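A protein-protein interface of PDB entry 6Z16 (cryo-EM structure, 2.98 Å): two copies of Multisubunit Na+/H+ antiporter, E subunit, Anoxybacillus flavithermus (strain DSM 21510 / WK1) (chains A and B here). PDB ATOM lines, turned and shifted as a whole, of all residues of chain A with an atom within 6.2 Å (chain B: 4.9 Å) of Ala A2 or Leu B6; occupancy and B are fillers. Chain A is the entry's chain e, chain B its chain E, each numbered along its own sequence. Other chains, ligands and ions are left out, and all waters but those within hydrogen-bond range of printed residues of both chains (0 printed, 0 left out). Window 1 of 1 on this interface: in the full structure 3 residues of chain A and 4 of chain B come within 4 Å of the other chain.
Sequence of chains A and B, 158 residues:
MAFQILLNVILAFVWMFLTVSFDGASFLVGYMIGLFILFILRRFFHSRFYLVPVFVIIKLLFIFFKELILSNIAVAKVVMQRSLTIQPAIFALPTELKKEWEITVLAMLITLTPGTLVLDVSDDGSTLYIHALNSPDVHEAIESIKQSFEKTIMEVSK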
ATOM      1  N   MET A   1       9.535 -23.567  15.585  1.00  0.00           N
ATOM      2  CA  MET A   1       8.223 -23.961  15.097  1.00  0.00           C
ATOM      3  C   MET A   1       7.418 -24.556  16.236  1.00  0.00           C
ATOM      4  O   MET A   1       6.197 -24.612  16.185  1.00  0.00           O
ATOM      5  CB  MET A   1       8.348 -24.966  13.957  1.00  0.00           C
ATOM      6  CG  MET A   1       9.027 -24.421  12.716  1.00  0.00           C
ATOM      7  SD  MET A   1       9.053 -25.618  11.370  1.00  0.00           S
ATOM      8  CE  MET A   1      10.273 -26.782  11.971  1.00  0.00           C
ATOM      9  N   ALA A   2       8.135 -25.025  17.256  1.00  0.00           N
ATOM     10  CA  ALA A   2       7.510 -25.502  18.481  1.00  0.00           C
ATOM     11  C   ALA A   2       7.508 -24.430  19.555  1.00  0.00           C
ATOM     12  O   ALA A   2       6.672 -24.468  20.466  1.00  0.00           O
ATOM     13  CB  ALA A   2       8.242 -26.740  18.987  1.00  0.00           C
ATOM     14  N   PHE A   3       8.443 -23.483  19.461  1.00  0.00           N
ATOM     15  CA  PHE A   3       8.485 -22.365  20.392  1.00  0.00           C
ATOM     16  C   PHE A   3       7.261 -21.480  20.238  1.00  0.00           C
ATOM     17  O   PHE A   3       6.716 -20.992  21.232  1.00  0.00           O
ATOM     18  CB  PHE A   3       9.760 -21.562  20.168  1.00  0.00           C
ATOM     19  CG  PHE A   3       9.916 -20.405  21.097  1.00  0.00           C
ATOM     20  CD1 PHE A   3      10.215 -20.613  22.429  1.00  0.00           C
ATOM     21  CD2 PHE A   3       9.802 -19.110  20.637  1.00  0.00           C
ATOM     22  CE1 PHE A   3      10.375 -19.550  23.292  1.00  0.00           C
ATOM     23  CE2 PHE A   3       9.966 -18.040  21.492  1.00  0.00           C
ATOM     24  CZ  PHE A   3      10.250 -18.261  22.824  1.00  0.00           C
ATOM     25  N   GLN A   4       6.791 -21.299  19.006  1.00  0.00           N
ATOM     26  CA  GLN A   4       5.586 -20.522  18.774  1.00  0.00           C
ATOM     27  C   GLN A   4       4.357 -21.238  19.301  1.00  0.00           C
ATOM     28  O   GLN A   4       3.441 -20.591  19.818  1.00  0.00           O
ATOM     29  CB  GLN A   4       5.431 -20.257  17.291  1.00  0.00           C
ATOM     30  CG  GLN A   4       6.637 -19.607  16.685  1.00  0.00           C
ATOM     31  CD  GLN A   4       6.468 -19.407  15.214  1.00  0.00           C
ATOM     32  OE1 GLN A   4       5.407 -19.678  14.667  1.00  0.00           O
ATOM     33  NE2 GLN A   4       7.528 -18.988  14.548  1.00  0.00           N
ATOM     34  N   ILE A   5       4.329 -22.566  19.210  1.00  0.00           N
ATOM     35  CA  ILE A   5       3.196 -23.315  19.737  1.00  0.00           C
ATOM     36  C   ILE A   5       3.178 -23.245  21.256  1.00  0.00           C
ATOM     37  O   ILE A   5       2.125 -23.031  21.869  1.00  0.00           O
ATOM     38  CB  ILE A   5       3.237 -24.766  19.235  1.00  0.00           C
ATOM     39  CG1 ILE A   5       3.236 -24.799  17.712  1.00  0.00           C
ATOM     40  CG2 ILE A   5       2.041 -25.532  19.736  1.00  0.00           C
ATOM     41  CD1 ILE A   5       3.466 -26.167  17.137  1.00  0.00           C
ATOM     42  N   LEU A   6       4.354 -23.377  21.880  1.00  0.00           N
ATOM     43  CA  LEU A   6       4.460 -23.248  23.332  1.00  0.00           C
ATOM     44  C   LEU A   6       4.110 -21.837  23.788  1.00  0.00           C
ATOM     45  O   LEU A   6       3.491 -21.646  24.844  1.00  0.00           O
ATOM     46  CB  LEU A   6       5.876 -23.610  23.778  1.00  0.00           C
ATOM     47  CG  LEU A   6       6.151 -23.531  25.277  1.00  0.00           C
ATOM     48  CD1 LEU A   6       5.371 -24.584  26.038  1.00  0.00           C
ATOM     49  CD2 LEU A   6       7.627 -23.626  25.552  1.00  0.00           C
ATOM     50  N   LEU A   7       4.466 -20.844  22.978  1.00  0.00           N
ATOM     51  CA  LEU A   7       4.200 -19.459  23.322  1.00  0.00           C
ATOM     52  C   LEU A   7       2.713 -19.162  23.221  1.00  0.00           C
ATOM     53  O   LEU A   7       2.160 -18.430  24.049  1.00  0.00           O
ATOM     54  CB  LEU A   7       5.021 -18.559  22.405  1.00  0.00           C
ATOM     55  CG  LEU A   7       5.383 -17.170  22.912  1.00  0.00           C
ATOM     56  CD1 LEU A   7       6.708 -16.793  22.318  1.00  0.00           C
ATOM     57  CD2 LEU A   7       4.350 -16.135  22.555  1.00  0.00           C
ATOM     58  N   VAL A   9       0.434 -21.479  23.754  1.00  0.00           N
ATOM     59  CA  VAL A   9      -0.158 -22.168  24.901  1.00  0.00           C
ATOM     60  C   VAL A   9      -0.013 -21.334  26.174  1.00  0.00           C
ATOM     61  O   VAL A   9      -0.966 -21.197  26.957  1.00  0.00           O
ATOM     62  CB  VAL A   9       0.457 -23.573  25.058  1.00  0.00           C
ATOM     63  CG1 VAL A   9       0.013 -24.225  26.359  1.00  0.00           C
ATOM     64  CG2 VAL A   9       0.034 -24.451  23.903  1.00  0.00           C
ATOM     65  N   ALA B   2      12.228 -25.917  23.882  1.00  0.00           N
ATOM     66  CA  ALA B   2      10.777 -25.831  23.899  1.00  0.00           C
ATOM     67  C   ALA B   2      10.128 -27.022  23.221  1.00  0.00           C
ATOM     68  O   ALA B   2       8.963 -27.327  23.501  1.00  0.00           O
ATOM     69  CB  ALA B   2      10.326 -24.547  23.215  1.00  0.00           C
ATOM     70  N   PHE B   3      10.864 -27.689  22.331  1.00  0.00           N
ATOM     71  CA  PHE B   3      10.355 -28.881  21.668  1.00  0.00           C
ATOM     72  C   PHE B   3      10.159 -30.014  22.659  1.00  0.00           C
ATOM     73  O   PHE B   3       9.188 -30.767  22.561  1.00  0.00           O
ATOM     74  CB  PHE B   3      11.309 -29.296  20.556  1.00  0.00           C
ATOM     75  CG  PHE B   3      10.850 -30.486  19.781  1.00  0.00           C
ATOM     76  CD1 PHE B   3       9.787 -30.386  18.905  1.00  0.00           C
ATOM     77  CD2 PHE B   3      11.503 -31.698  19.898  1.00  0.00           C
ATOM     78  CE1 PHE B   3       9.364 -31.479  18.176  1.00  0.00           C
ATOM     79  CE2 PHE B   3      11.092 -32.793  19.166  1.00  0.00           C
ATOM     80  CZ  PHE B   3      10.020 -32.685  18.307  1.00  0.00           C
ATOM     81  N   GLN B   4      11.050 -30.122  23.643  1.00  0.00           N
ATOM     82  CA  GLN B   4      10.905 -31.141  24.670  1.00  0.00           C
ATOM     83  C   GLN B   4       9.716 -30.847  25.565  1.00  0.00           C
ATOM     84  O   GLN B   4       9.017 -31.769  25.999  1.00  0.00           O
ATOM     85  CB  GLN B   4      12.172 -31.211  25.500  1.00  0.00           C
ATOM     86  CG  GLN B   4      13.406 -31.429  24.684  1.00  0.00           C
ATOM     87  CD  GLN B   4      14.626 -31.444  25.545  1.00  0.00           C
ATOM     88  OE1 GLN B   4      14.526 -31.380  26.765  1.00  0.00           O
ATOM     89  NE2 GLN B   4      15.792 -31.472  24.926  1.00  0.00           N
ATOM     90  N   ILE B   5       9.454 -29.569  25.833  1.00  0.00           N
ATOM     91  CA  ILE B   5       8.312 -29.216  26.664  1.00  0.00           C
ATOM     92  C   ILE B   5       7.016 -29.498  25.922  1.00  0.00           C
ATOM     93  O   ILE B   5       6.070 -30.060  26.487  1.00  0.00           O
ATOM     94  CB  ILE B   5       8.403 -27.747  27.103  1.00  0.00           C
ATOM     95  CG1 ILE B   5       9.733 -27.486  27.796  1.00  0.00           C
ATOM     96  CG2 ILE B   5       7.287 -27.420  28.064  1.00  0.00           C
ATOM     97  CD1 ILE B   5       9.985 -26.039  28.090  1.00  0.00           C
ATOM     98  N   LEU B   6       6.972 -29.156  24.630  1.00  0.00           N
ATOM     99  CA  LEU B   6       5.812 -29.466  23.798  1.00  0.00           C
ATOM    100  C   LEU B   6       5.616 -30.970  23.660  1.00  0.00           C
ATOM    101  O   LEU B   6       4.479 -31.462  23.631  1.00  0.00           O
ATOM    102  CB  LEU B   6       5.982 -28.826  22.420  1.00  0.00           C
ATOM    103  CG  LEU B   6       4.845 -29.050  21.429  1.00  0.00           C
ATOM    104  CD1 LEU B   6       3.580 -28.350  21.878  1.00  0.00           C
ATOM    105  CD2 LEU B   6       5.253 -28.620  20.046  1.00  0.00           C
ATOM    106  N   LEU B   7       6.718 -31.714  23.614  1.00  0.00           N
ATOM    107  CA  LEU B   7       6.649 -33.155  23.463  1.00  0.00           C
ATOM    108  C   LEU B   7       6.127 -33.802  24.738  1.00  0.00           C
ATOM    109  O   LEU B   7       5.350 -34.759  24.683  1.00  0.00           O
ATOM    110  CB  LEU B   7       8.031 -33.679  23.089  1.00  0.00           C
ATOM    111  CG  LEU B   7       8.112 -34.992  22.319  1.00  0.00           C
ATOM    112  CD1 LEU B   7       9.327 -34.939  21.437  1.00  0.00           C
ATOM    113  CD2 LEU B   7       8.190 -36.192  23.225  1.00  0.00           C
ATOM    114  N   ASN B   8       6.513 -33.256  25.892  1.00  0.00           N
ATOM    115  CA  ASN B   8       5.972 -33.722  27.164  1.00  0.00           C
ATOM    116  C   ASN B   8       4.484 -33.402  27.283  1.00  0.00           C
ATOM    117  O   ASN B   8       3.712 -34.210  27.820  1.00  0.00           O
ATOM    118  CB  ASN B   8       6.767 -33.088  28.304  1.00  0.00           C
ATOM    119  CG  ASN B   8       6.764 -33.919  29.575  1.00  0.00           C
ATOM    120  OD1 ASN B   8       7.624 -33.737  30.433  1.00  0.00           O
ATOM    121  ND2 ASN B   8       5.798 -34.820  29.715  1.00  0.00           N
ATOM    122  N   VAL B   9       4.061 -32.244  26.765  1.00  0.00           N
ATOM    123  CA  VAL B   9       2.639 -31.894  26.793  1.00  0.00           C
ATOM    124  C   VAL B   9       1.826 -32.837  25.906  1.00  0.00           C
ATOM    125  O   VAL B   9       0.755 -33.321  26.304  1.00  0.00           O
ATOM    126  CB  VAL B   9       2.445 -30.419  26.395  1.00  0.00           C
ATOM    127  CG1 VAL B   9       0.972 -30.089  26.216  1.00  0.00           C
ATOM    128  CG2 VAL B   9       3.022 -29.516  27.461  1.00  0.00           C
ATOM    129  N   ILE B  10       2.336 -33.159  24.716  1.00  0.00           N
ATOM    130  CA  ILE B  10       1.546 -34.029  23.850  1.00  0.00           C
ATOM    131  C   ILE B  10       1.610 -35.485  24.316  1.00  0.00           C
ATOM    132  O   ILE B  10       0.665 -36.242  24.084  1.00  0.00           O
ATOM    133  CB  ILE B  10       1.939 -33.857  22.366  1.00  0.00           C
ATOM    134  CG1 ILE B  10       3.393 -34.237  22.072  1.00  0.00           C
ATOM    135  CG2 ILE B  10       1.675 -32.430  21.911  1.00  0.00           C
ATOM    136  CD1 ILE B  10       3.590 -35.631  21.493  1.00  0.00           C
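Among the printed residues, merely in contact across the chains: Ala A2 with Phe B3 (3.96 Å), Ala A2 with Leu B6 (3.7 Å), Ile A5 with Leu B6 (3.9 Å), Leu A6 with Ala B2 (3.7 Å) and Leu A6 with Ile B5 (3.98 Å).
Ala A2 touches Phe B3, but with the chains exchanged Phe A3 does not touch Ala B2 (4.01 Å). Ala A2 touches Leu B6, and with the chains exchanged Leu A6 touches Ala B2. Ile A5 touches Leu B6, and with the chains exchanged Leu A6 touches Ile B5. Positions printed for both chains: 2, 3, 4, 5, 6, 7 and 9. Of the 5 pairs that touch across the chains among the printed residues, 4 have their exchanged pair printed and touching as well.
Of the 8 printed residues of chain A, 3 touch a printed residue of chain B. Hydrophobic or aromatic side chains of chain A that line the printed part of chain B: Ala A2, Ile A5 and Leu A6. Among the printed residues, 5 pairs touch across the chains.
Of chain B, only Phe B3 and Leu B6 come within 4 Å of Ala A2. Phe A3 touches none of the printed residues of chain B. Of the printed residues of chain A, Ala B2 touches Leu A6. Printed residues of chain A within 4 Å of Phe B3: Ala A2 (3.96 Å). Of the printed residues of chain A, Ile B5 touches Leu A6. Of chain A, only Ala A2 (3.7 Å) and Ile A5 (3.9 Å) come within 4 Å of Leu B6. The nearest residue of chain B that does not touch Ala A2 is Ala B2 (4.6 Å).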
